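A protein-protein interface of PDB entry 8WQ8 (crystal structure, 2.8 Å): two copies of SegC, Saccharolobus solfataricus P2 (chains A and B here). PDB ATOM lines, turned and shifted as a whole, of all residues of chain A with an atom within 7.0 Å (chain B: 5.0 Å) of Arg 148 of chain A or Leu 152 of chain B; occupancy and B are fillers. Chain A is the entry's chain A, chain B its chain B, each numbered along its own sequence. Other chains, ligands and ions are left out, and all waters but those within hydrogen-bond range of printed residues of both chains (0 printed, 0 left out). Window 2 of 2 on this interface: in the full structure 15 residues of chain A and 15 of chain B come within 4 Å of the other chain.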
ATOM      1  N   TYR A  11     -12.476  -4.239  30.264  1.00  0.00           N
ATOM      2  CA  TYR A  11     -13.366  -5.393  30.167  1.00  0.00           C
ATOM      3  C   TYR A  11     -14.022  -5.721  31.510  1.00  0.00           C
ATOM      4  O   TYR A  11     -15.239  -5.938  31.582  1.00  0.00           O
ATOM      5  CB  TYR A  11     -12.591  -6.592  29.631  1.00  0.00           C
ATOM      6  CG  TYR A  11     -12.643  -6.685  28.126  1.00  0.00           C
ATOM      7  CD1 TYR A  11     -11.899  -5.810  27.336  1.00  0.00           C
ATOM      8  CD2 TYR A  11     -13.440  -7.635  27.491  1.00  0.00           C
ATOM      9  CE1 TYR A  11     -11.938  -5.878  25.973  1.00  0.00           C
ATOM     10  CE2 TYR A  11     -13.479  -7.712  26.116  1.00  0.00           C
ATOM     11  CZ  TYR A  11     -12.725  -6.830  25.359  1.00  0.00           C
ATOM     12  OH  TYR A  11     -12.772  -6.897  23.982  1.00  0.00           O
ATOM     13  N   GLU A  14     -16.740  -3.238  32.214  1.00  0.00           N
ATOM     14  CA  GLU A  14     -17.976  -3.491  31.483  1.00  0.00           C
ATOM     15  C   GLU A  14     -18.738  -4.679  32.076  1.00  0.00           C
ATOM     16  O   GLU A  14     -19.960  -4.608  32.263  1.00  0.00           O
ATOM     17  CB  GLU A  14     -17.693  -3.705  29.991  1.00  0.00           C
ATOM     18  CG  GLU A  14     -17.410  -2.422  29.163  1.00  0.00           C
ATOM     19  CD  GLU A  14     -18.460  -1.315  29.341  1.00  0.00           C
ATOM     20  OE1 GLU A  14     -19.673  -1.576  29.160  1.00  0.00           O
ATOM     21  OE2 GLU A  14     -18.061  -0.170  29.645  1.00  0.00           O
ATOM     22  N   PHE A  15     -18.030  -5.766  32.413  1.00  0.00           N
ATOM     23  CA  PHE A  15     -18.715  -6.947  32.931  1.00  0.00           C
ATOM     24  C   PHE A  15     -19.374  -6.662  34.276  1.00  0.00           C
ATOM     25  O   PHE A  15     -20.480  -7.159  34.550  1.00  0.00           O
ATOM     26  CB  PHE A  15     -17.756  -8.129  33.054  1.00  0.00           C
ATOM     27  CG  PHE A  15     -18.368  -9.329  33.736  1.00  0.00           C
ATOM     28  CD1 PHE A  15     -19.298 -10.126  33.068  1.00  0.00           C
ATOM     29  CD2 PHE A  15     -18.028  -9.649  35.054  1.00  0.00           C
ATOM     30  CE1 PHE A  15     -19.879 -11.219  33.691  1.00  0.00           C
ATOM     31  CE2 PHE A  15     -18.608 -10.742  35.694  1.00  0.00           C
ATOM     32  CZ  PHE A  15     -19.532 -11.536  35.009  1.00  0.00           C
ATOM     33  N   LYS A  17     -20.608  -3.772  35.297  1.00  0.00           N
ATOM     34  CA  LYS A  17     -21.849  -3.049  35.037  1.00  0.00           C
ATOM     35  C   LYS A  17     -22.963  -4.014  34.632  1.00  0.00           C
ATOM     36  O   LYS A  17     -24.106  -3.879  35.082  1.00  0.00           O
ATOM     37  CB  LYS A  17     -21.639  -1.993  33.963  1.00  0.00           C
ATOM     38  CG  LYS A  17     -20.704  -0.873  34.359  1.00  0.00           C
ATOM     39  CD  LYS A  17     -20.651   0.111  33.218  1.00  0.00           C
ATOM     40  CE  LYS A  17     -19.438   1.011  33.223  1.00  0.00           C
ATOM     41  NZ  LYS A  17     -19.323   1.618  31.858  1.00  0.00           N
ATOM     42  N   ILE A  18     -22.644  -5.015  33.807  1.00  0.00           N
ATOM     43  CA  ILE A  18     -23.648  -6.006  33.449  1.00  0.00           C
ATOM     44  C   ILE A  18     -24.059  -6.823  34.668  1.00  0.00           C
ATOM     45  O   ILE A  18     -25.245  -7.112  34.865  1.00  0.00           O
ATOM     46  CB  ILE A  18     -23.125  -6.888  32.305  1.00  0.00           C
ATOM     47  CG1 ILE A  18     -23.072  -6.054  31.028  1.00  0.00           C
ATOM     48  CG2 ILE A  18     -23.998  -8.154  32.136  1.00  0.00           C
ATOM     49  CD1 ILE A  18     -22.044  -6.501  30.048  1.00  0.00           C
ATOM     50  N   ASN A 141     -14.173   4.542  24.434  1.00  0.00           N
ATOM     51  CA  ASN A 141     -15.585   4.309  24.128  1.00  0.00           C
ATOM     52  C   ASN A 141     -15.759   3.228  23.070  1.00  0.00           C
ATOM     53  O   ASN A 141     -16.685   2.414  23.153  1.00  0.00           O
ATOM     54  CB  ASN A 141     -16.247   5.601  23.672  1.00  0.00           C
ATOM     55  CG  ASN A 141     -16.856   6.370  24.819  1.00  0.00           C
ATOM     56  OD1 ASN A 141     -17.013   5.838  25.922  1.00  0.00           O
ATOM     57  ND2 ASN A 141     -17.177   7.643  24.580  1.00  0.00           N
ATOM     58  N   ILE A 143     -13.650   0.794  22.572  1.00  0.00           N
ATOM     59  CA  ILE A 143     -13.221  -0.443  23.205  1.00  0.00           C
ATOM     60  C   ILE A 143     -14.321  -0.991  24.101  1.00  0.00           C
ATOM     61  O   ILE A 143     -14.590  -2.195  24.102  1.00  0.00           O
ATOM     62  CB  ILE A 143     -11.924  -0.193  23.982  1.00  0.00           C
ATOM     63  CG1 ILE A 143     -10.810   0.100  22.981  1.00  0.00           C
ATOM     64  CG2 ILE A 143     -11.589  -1.393  24.850  1.00  0.00           C
ATOM     65  CD1 ILE A 143      -9.426  -0.172  23.482  1.00  0.00           C
ATOM     66  N   ARG A 144     -14.980  -0.118  24.868  1.00  0.00           N
ATOM     67  CA  ARG A 144     -16.090  -0.563  25.704  1.00  0.00           C
ATOM     68  C   ARG A 144     -17.190  -1.222  24.881  1.00  0.00           C
ATOM     69  O   ARG A 144     -17.705  -2.281  25.270  1.00  0.00           O
ATOM     70  CB  ARG A 144     -16.658   0.602  26.501  1.00  0.00           C
ATOM     71  CG  ARG A 144     -15.666   1.235  27.403  1.00  0.00           C
ATOM     72  CD  ARG A 144     -16.337   2.160  28.367  1.00  0.00           C
ATOM     73  NE  ARG A 144     -15.367   2.754  29.271  1.00  0.00           N
ATOM     74  CZ  ARG A 144     -15.320   2.495  30.566  1.00  0.00           C
ATOM     75  NH1 ARG A 144     -16.147   1.623  31.123  1.00  0.00           N
ATOM     76  NH2 ARG A 144     -14.423   3.121  31.321  1.00  0.00           N
ATOM     77  N   LEU A 145     -17.567  -0.621  23.740  1.00  0.00           N
ATOM     78  CA  LEU A 145     -18.647  -1.203  22.948  1.00  0.00           C
ATOM     79  C   LEU A 145     -18.254  -2.579  22.414  1.00  0.00           C
ATOM     80  O   LEU A 145     -19.077  -3.505  22.410  1.00  0.00           O
ATOM     81  CB  LEU A 145     -19.058  -0.266  21.810  1.00  0.00           C
ATOM     82  CG  LEU A 145     -20.246  -0.697  20.924  1.00  0.00           C
ATOM     83  CD1 LEU A 145     -19.789  -1.511  19.702  1.00  0.00           C
ATOM     84  CD2 LEU A 145     -21.330  -1.469  21.699  1.00  0.00           C
ATOM     85  N   ILE A 146     -17.003  -2.745  21.978  1.00  0.00           N
ATOM     86  CA  ILE A 146     -16.549  -4.079  21.582  1.00  0.00           C
ATOM     87  C   ILE A 146     -16.586  -5.022  22.780  1.00  0.00           C
ATOM     88  O   ILE A 146     -17.084  -6.151  22.686  1.00  0.00           O
ATOM     89  CB  ILE A 146     -15.142  -4.025  20.961  1.00  0.00           C
ATOM     90  CG1 ILE A 146     -15.197  -3.481  19.537  1.00  0.00           C
ATOM     91  CG2 ILE A 146     -14.568  -5.416  20.911  1.00  0.00           C
ATOM     92  CD1 ILE A 146     -13.953  -2.723  19.120  1.00  0.00           C
ATOM     93  N   ALA A 147     -16.081  -4.565  23.929  1.00  0.00           N
ATOM     94  CA  ALA A 147     -16.072  -5.398  25.124  1.00  0.00           C
ATOM     95  C   ALA A 147     -17.479  -5.844  25.489  1.00  0.00           C
ATOM     96  O   ALA A 147     -17.704  -7.020  25.797  1.00  0.00           O
ATOM     97  CB  ALA A 147     -15.426  -4.647  26.287  1.00  0.00           C
ATOM     98  N   ARG A 148     -18.440  -4.919  25.462  1.00  0.00           N
ATOM     99  CA  ARG A 148     -19.813  -5.285  25.794  1.00  0.00           C
ATOM    100  C   ARG A 148     -20.321  -6.394  24.885  1.00  0.00           C
ATOM    101  O   ARG A 148     -20.894  -7.383  25.358  1.00  0.00           O
ATOM    102  CB  ARG A 148     -20.730  -4.071  25.703  1.00  0.00           C
ATOM    103  CG  ARG A 148     -21.271  -3.679  27.036  1.00  0.00           C
ATOM    104  CD  ARG A 148     -22.303  -2.586  26.939  1.00  0.00           C
ATOM    105  NE  ARG A 148     -22.019  -1.670  25.850  1.00  0.00           N
ATOM    106  CZ  ARG A 148     -21.584  -0.431  26.021  1.00  0.00           C
ATOM    107  NH1 ARG A 148     -21.342   0.052  27.227  1.00  0.00           N
ATOM    108  NH2 ARG A 148     -21.396   0.343  24.956  1.00  0.00           N
ATOM    109  N   LYS A 149     -20.122  -6.245  23.569  1.00  0.00           N
ATOM    110  CA  LYS A 149     -20.609  -7.253  22.634  1.00  0.00           C
ATOM    111  C   LYS A 149     -19.937  -8.590  22.887  1.00  0.00           C
ATOM    112  O   LYS A 149     -20.590  -9.642  22.842  1.00  0.00           O
ATOM    113  CB  LYS A 149     -20.378  -6.793  21.194  1.00  0.00           C
ATOM    114  CG  LYS A 149     -21.231  -5.596  20.819  1.00  0.00           C
ATOM    115  CD  LYS A 149     -21.273  -5.366  19.328  1.00  0.00           C
ATOM    116  CE  LYS A 149     -21.966  -4.056  19.034  1.00  0.00           C
ATOM    117  NZ  LYS A 149     -21.558  -3.514  17.708  1.00  0.00           N
ATOM    118  N   GLU A 150     -18.631  -8.563  23.173  1.00  0.00           N
ATOM    119  CA  GLU A 150     -17.889  -9.796  23.399  1.00  0.00           C
ATOM    120  C   GLU A 150     -18.288 -10.458  24.716  1.00  0.00           C
ATOM    121  O   GLU A 150     -18.397 -11.689  24.786  1.00  0.00           O
ATOM    122  CB  GLU A 150     -16.396  -9.508  23.371  1.00  0.00           C
ATOM    123  CG  GLU A 150     -15.740 -10.000  22.120  1.00  0.00           C
ATOM    124  CD  GLU A 150     -14.483  -9.235  21.793  1.00  0.00           C
ATOM    125  OE1 GLU A 150     -14.250  -8.970  20.591  1.00  0.00           O
ATOM    126  OE2 GLU A 150     -13.722  -8.925  22.737  1.00  0.00           O
ATOM    127  N   ILE A 151     -18.512  -9.666  25.772  1.00  0.00           N
ATOM    128  CA  ILE A 151     -18.990 -10.234  27.033  1.00  0.00           C
ATOM    129  C   ILE A 151     -20.380 -10.832  26.849  1.00  0.00           C
ATOM    130  O   ILE A 151     -20.661 -11.940  27.321  1.00  0.00           O
ATOM    131  CB  ILE A 151     -18.988  -9.175  28.148  1.00  0.00           C
ATOM    132  CG1 ILE A 151     -17.576  -8.915  28.651  1.00  0.00           C
ATOM    133  CG2 ILE A 151     -19.872  -9.623  29.291  1.00  0.00           C
ATOM    134  CD1 ILE A 151     -17.410  -7.508  29.171  1.00  0.00           C
ATOM    135  N   LEU A 152     -21.272 -10.100  26.166  1.00  0.00           N
ATOM    136  CA  LEU A 152     -22.628 -10.594  25.927  1.00  0.00           C
ATOM    137  C   LEU A 152     -22.614 -11.896  25.139  1.00  0.00           C
ATOM    138  O   LEU A 152     -23.423 -12.798  25.392  1.00  0.00           O
ATOM    139  CB  LEU A 152     -23.462  -9.546  25.188  1.00  0.00           C
ATOM    140  CG  LEU A 152     -24.948  -9.906  25.093  1.00  0.00           C
ATOM    141  CD1 LEU A 152     -25.487 -10.249  26.474  1.00  0.00           C
ATOM    142  CD2 LEU A 152     -25.745  -8.786  24.484  1.00  0.00           C
ATOM    143  N   GLU A 153     -21.706 -12.006  24.168  1.00  0.00           N
ATOM    144  CA  GLU A 153     -21.548 -13.262  23.454  1.00  0.00           C
ATOM    145  C   GLU A 153     -21.144 -14.377  24.408  1.00  0.00           C
ATOM    146  O   GLU A 153     -21.627 -15.511  24.299  1.00  0.00           O
ATOM    147  CB  GLU A 153     -20.512 -13.092  22.351  1.00  0.00           C
ATOM    148  CG  GLU A 153     -20.235 -14.356  21.580  1.00  0.00           C
ATOM    149  CD  GLU A 153     -19.348 -14.109  20.374  1.00  0.00           C
ATOM    150  OE1 GLU A 153     -18.255 -13.514  20.550  1.00  0.00           O
ATOM    151  OE2 GLU A 153     -19.749 -14.498  19.251  1.00  0.00           O
ATOM    152  N   ARG A 154     -20.262 -14.070  25.360  1.00  0.00           N
ATOM    153  CA  ARG A 154     -19.848 -15.076  26.325  1.00  0.00           C
ATOM    154  C   ARG A 154     -21.016 -15.507  27.195  1.00  0.00           C
ATOM    155  O   ARG A 154     -21.246 -16.710  27.390  1.00  0.00           O
ATOM    156  CB  ARG A 154     -18.711 -14.542  27.195  1.00  0.00           C
ATOM    157  CG  ARG A 154     -18.013 -15.631  27.944  1.00  0.00           C
ATOM    158  CD  ARG A 154     -17.770 -16.761  26.995  1.00  0.00           C
ATOM    159  NE  ARG A 154     -16.501 -16.583  26.306  1.00  0.00           N
ATOM    160  CZ  ARG A 154     -15.324 -16.921  26.820  1.00  0.00           C
ATOM    161  NH1 ARG A 154     -15.227 -17.508  28.009  1.00  0.00           N
ATOM    162  NH2 ARG A 154     -14.220 -16.670  26.124  1.00  0.00           N
ATOM    163  N   ILE A 155     -21.748 -14.534  27.747  1.00  0.00           N
ATOM    164  CA  ILE A 155     -22.846 -14.849  28.648  1.00  0.00           C
ATOM    165  C   ILE A 155     -23.883 -15.690  27.928  1.00  0.00           C
ATOM    166  O   ILE A 155     -24.435 -16.638  28.498  1.00  0.00           O
ATOM    167  CB  ILE A 155     -23.455 -13.561  29.231  1.00  0.00           C
ATOM    168  CG1 ILE A 155     -22.381 -12.749  29.970  1.00  0.00           C
ATOM    169  CG2 ILE A 155     -24.637 -13.901  30.142  1.00  0.00           C
ATOM    170  CD1 ILE A 155     -22.844 -11.376  30.446  1.00  0.00           C
ATOM    171  N   ALA B 147     -32.277  -4.994  19.689  1.00  0.00           N
ATOM    172  CA  ALA B 147     -32.846  -5.654  20.857  1.00  0.00           C
ATOM    173  C   ALA B 147     -31.756  -6.012  21.860  1.00  0.00           C
ATOM    174  O   ALA B 147     -31.928  -5.832  23.074  1.00  0.00           O
ATOM    175  CB  ALA B 147     -33.624  -6.899  20.422  1.00  0.00           C
ATOM    176  N   ARG B 148     -30.617  -6.505  21.362  1.00  0.00           N
ATOM    177  CA  ARG B 148     -29.487  -6.813  22.226  1.00  0.00           C
ATOM    178  C   ARG B 148     -29.021  -5.584  22.981  1.00  0.00           C
ATOM    179  O   ARG B 148     -28.806  -5.634  24.197  1.00  0.00           O
ATOM    180  CB  ARG B 148     -28.346  -7.380  21.399  1.00  0.00           C
ATOM    181  CG  ARG B 148     -28.148  -8.842  21.583  1.00  0.00           C
ATOM    182  CD  ARG B 148     -27.040  -9.275  20.706  1.00  0.00           C
ATOM    183  NE  ARG B 148     -27.587  -9.942  19.541  1.00  0.00           N
ATOM    184  CZ  ARG B 148     -27.158  -9.746  18.304  1.00  0.00           C
ATOM    185  NH1 ARG B 148     -26.190  -8.884  18.037  1.00  0.00           N
ATOM    186  NH2 ARG B 148     -27.711 -10.438  17.313  1.00  0.00           N
ATOM    187  N   LYS B 149     -28.838  -4.470  22.270  1.00  0.00           N
ATOM    188  CA  LYS B 149     -28.352  -3.272  22.937  1.00  0.00           C
ATOM    189  C   LYS B 149     -29.345  -2.816  23.994  1.00  0.00           C
ATOM    190  O   LYS B 149     -28.952  -2.430  25.103  1.00  0.00           O
ATOM    191  CB  LYS B 149     -28.087  -2.163  21.923  1.00  0.00           C
ATOM    192  CG  LYS B 149     -28.044  -0.763  22.547  1.00  0.00           C
ATOM    193  CD  LYS B 149     -28.449   0.350  21.563  1.00  0.00           C
ATOM    194  CE  LYS B 149     -28.758   1.676  22.285  1.00  0.00           C
ATOM    195  NZ  LYS B 149     -29.436   1.511  23.621  1.00  0.00           N
ATOM    196  N   GLU B 150     -30.640  -2.893  23.687  1.00  0.00           N
ATOM    197  CA  GLU B 150     -31.641  -2.398  24.622  1.00  0.00           C
ATOM    198  C   GLU B 150     -31.905  -3.392  25.747  1.00  0.00           C
ATOM    199  O   GLU B 150     -32.179  -2.982  26.878  1.00  0.00           O
ATOM    200  CB  GLU B 150     -32.935  -2.069  23.885  1.00  0.00           C
ATOM    201  CG  GLU B 150     -32.740  -1.090  22.769  1.00  0.00           C
ATOM    202  CD  GLU B 150     -34.034  -0.739  22.057  1.00  0.00           C
ATOM    203  OE1 GLU B 150     -35.069  -1.420  22.290  1.00  0.00           O
ATOM    204  OE2 GLU B 150     -34.002   0.231  21.263  1.00  0.00           O
ATOM    205  N   ILE B 151     -31.839  -4.696  25.464  1.00  0.00           N
ATOM    206  CA  ILE B 151     -31.951  -5.673  26.543  1.00  0.00           C
ATOM    207  C   ILE B 151     -30.780  -5.530  27.503  1.00  0.00           C
ATOM    208  O   ILE B 151     -30.963  -5.429  28.722  1.00  0.00           O
ATOM    209  CB  ILE B 151     -32.035  -7.102  25.988  1.00  0.00           C
ATOM    210  CG1 ILE B 151     -33.380  -7.337  25.305  1.00  0.00           C
ATOM    211  CG2 ILE B 151     -31.801  -8.108  27.111  1.00  0.00           C
ATOM    212  CD1 ILE B 151     -33.345  -8.511  24.337  1.00  0.00           C
ATOM    213  N   LEU B 152     -29.552  -5.506  26.958  1.00  0.00           N
ATOM    214  CA  LEU B 152     -28.370  -5.353  27.798  1.00  0.00           C
ATOM    215  C   LEU B 152     -28.433  -4.067  28.600  1.00  0.00           C
ATOM    216  O   LEU B 152     -28.075  -4.048  29.783  1.00  0.00           O
ATOM    217  CB  LEU B 152     -27.100  -5.378  26.957  1.00  0.00           C
ATOM    218  CG  LEU B 152     -25.844  -5.591  27.808  1.00  0.00           C
ATOM    219  CD1 LEU B 152     -25.877  -6.969  28.449  1.00  0.00           C
ATOM    220  CD2 LEU B 152     -24.560  -5.395  27.014  1.00  0.00           C
ATOM    221  N   GLU B 153     -28.896  -2.979  27.975  1.00  0.00           N
ATOM    222  CA  GLU B 153     -29.050  -1.720  28.700  1.00  0.00           C
ATOM    223  C   GLU B 153     -30.009  -1.883  29.873  1.00  0.00           C
ATOM    224  O   GLU B 153     -29.734  -1.412  30.980  1.00  0.00           O
ATOM    225  CB  GLU B 153     -29.518  -0.626  27.743  1.00  0.00           C
ATOM    226  CG  GLU B 153     -30.353   0.487  28.363  1.00  0.00           C
ATOM    227  CD  GLU B 153     -30.342   1.771  27.516  1.00  0.00           C
ATOM    228  OE1 GLU B 153     -30.504   1.672  26.267  1.00  0.00           O
ATOM    229  OE2 GLU B 153     -30.183   2.875  28.100  1.00  0.00           O
ATOM    230  N   ARG B 154     -31.110  -2.602  29.666  1.00  0.00           N
ATOM    231  CA  ARG B 154     -32.061  -2.821  30.748  1.00  0.00           C
ATOM    232  C   ARG B 154     -31.452  -3.665  31.866  1.00  0.00           C
ATOM    233  O   ARG B 154     -31.527  -3.298  33.045  1.00  0.00           O
ATOM    234  CB  ARG B 154     -33.320  -3.476  30.195  1.00  0.00           C
ATOM    235  CG  ARG B 154     -34.312  -3.807  31.261  1.00  0.00           C
ATOM    236  CD  ARG B 154     -34.928  -2.541  31.768  1.00  0.00           C
ATOM    237  NE  ARG B 154     -35.550  -1.806  30.676  1.00  0.00           N
ATOM    238  CZ  ARG B 154     -36.837  -1.494  30.658  1.00  0.00           C
ATOM    239  NH1 ARG B 154     -37.643  -1.856  31.646  1.00  0.00           N
ATOM    240  NH2 ARG B 154     -37.327  -0.825  29.618  1.00  0.00           N
ATOM    241  N   ILE B 155     -30.852  -4.806  31.510  1.00  0.00           N
ATOM    242  CA  ILE B 155     -30.169  -5.668  32.482  1.00  0.00           C
ATOM    243  C   ILE B 155     -29.161  -4.875  33.322  1.00  0.00           C
ATOM    244  O   ILE B 155     -29.121  -4.988  34.553  1.00  0.00           O
ATOM    245  CB  ILE B 155     -29.472  -6.827  31.754  1.00  0.00           C
ATOM    246  CG1 ILE B 155     -30.497  -7.787  31.166  1.00  0.00           C
ATOM    247  CG2 ILE B 155     -28.533  -7.527  32.695  1.00  0.00           C
ATOM    248  CD1 ILE B 155     -29.866  -8.898  30.345  1.00  0.00           C
ATOM    249  N   SER B 156     -28.325  -4.069  32.664  1.00  0.00           N
ATOM    250  CA  SER B 156     -27.251  -3.357  33.345  1.00  0.00           C
ATOM    251  C   SER B 156     -27.743  -2.274  34.300  1.00  0.00           C
ATOM    252  O   SER B 156     -26.918  -1.680  35.003  1.00  0.00           O
ATOM    253  CB  SER B 156     -26.313  -2.723  32.319  1.00  0.00           C
ATOM    254  OG  SER B 156     -25.755  -3.707  31.471  1.00  0.00           O
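Among the printed residues, pairs that only touch across the chains: Lys 17 of chain A with Ser 156 of chain B, Ile 18 of chain A with Leu 152 of chain B, Ile 18 of chain A with Ile 155 of chain B, Ile 18 of chain A with Ser 156 of chain B, Arg 148 of chain A with Leu 152 of chain B, Leu 152 of chain A with Arg 148 of chain B and Leu 152 of chain A with Leu 152 of chain B.
The side-chain carboxylate of Glu 14 of chain A lies within salt-bridge range of the guanidinium group of Arg 148 of chain A (3.0 Å). The side-chain carboxylate (OE2) of Glu 14 of chain A is in salt-bridge range of the side-chain amino group (NZ) of Lys 17 of chain A (3.1 Å). The backbone carbonyl oxygen (O) of Leu 152 of chain B lies within hydrogen-bond range of the side-chain hydroxyl (OG) of Ser 156 of chain B, at 2.9 Å.
Arg 148 of chain A touches Leu 152 of chain B, and with the chains exchanged Leu 152 of chain A touches Arg 148 of chain B. Leu 152 of chain B touches its own counterpart, Leu 152 of chain A. 9 positions are printed for both chains.
Printed residues of chain A that touch a printed residue of chain B: Lys 17, Ile 18, Arg 148 and Leu 152. Hydrophobic or aromatic side chains of chain A that line the printed part of chain B: Ile 18 and Leu 152. Hydrophobic or aromatic side chains of chain B within 4 Å of the printed part of chain A: Leu 152 and Ile 155. Among the printed residues, no Asp or Glu carboxylate lies within 4 Å of a Lys or Arg side-chain nitrogen of the other chain.
Of chain B, only Leu 152 comes within 4 Å of Arg 148 of chain A. Of chain A, only Ile 18 (3.9 Å), Arg 148 (3.6 Å) and Leu 152 (3.8 Å) come within 4 Å of Leu 152 of chain B. Printed residues of chain A within 4 Å of Ile 155 of chain B: Ile 18 (3.96 Å). Of the printed residues of chain A, Arg 148 of chain B touches Leu 152. Of the printed residues of chain B, Ile 18 of chain A touches Leu 152 (3.9 Å), Ile 155 (3.96 Å) and Ser 156 (3.6 Å). Printed residues of chain B within 4 Å of Lys 17 of chain A: Ser 156.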
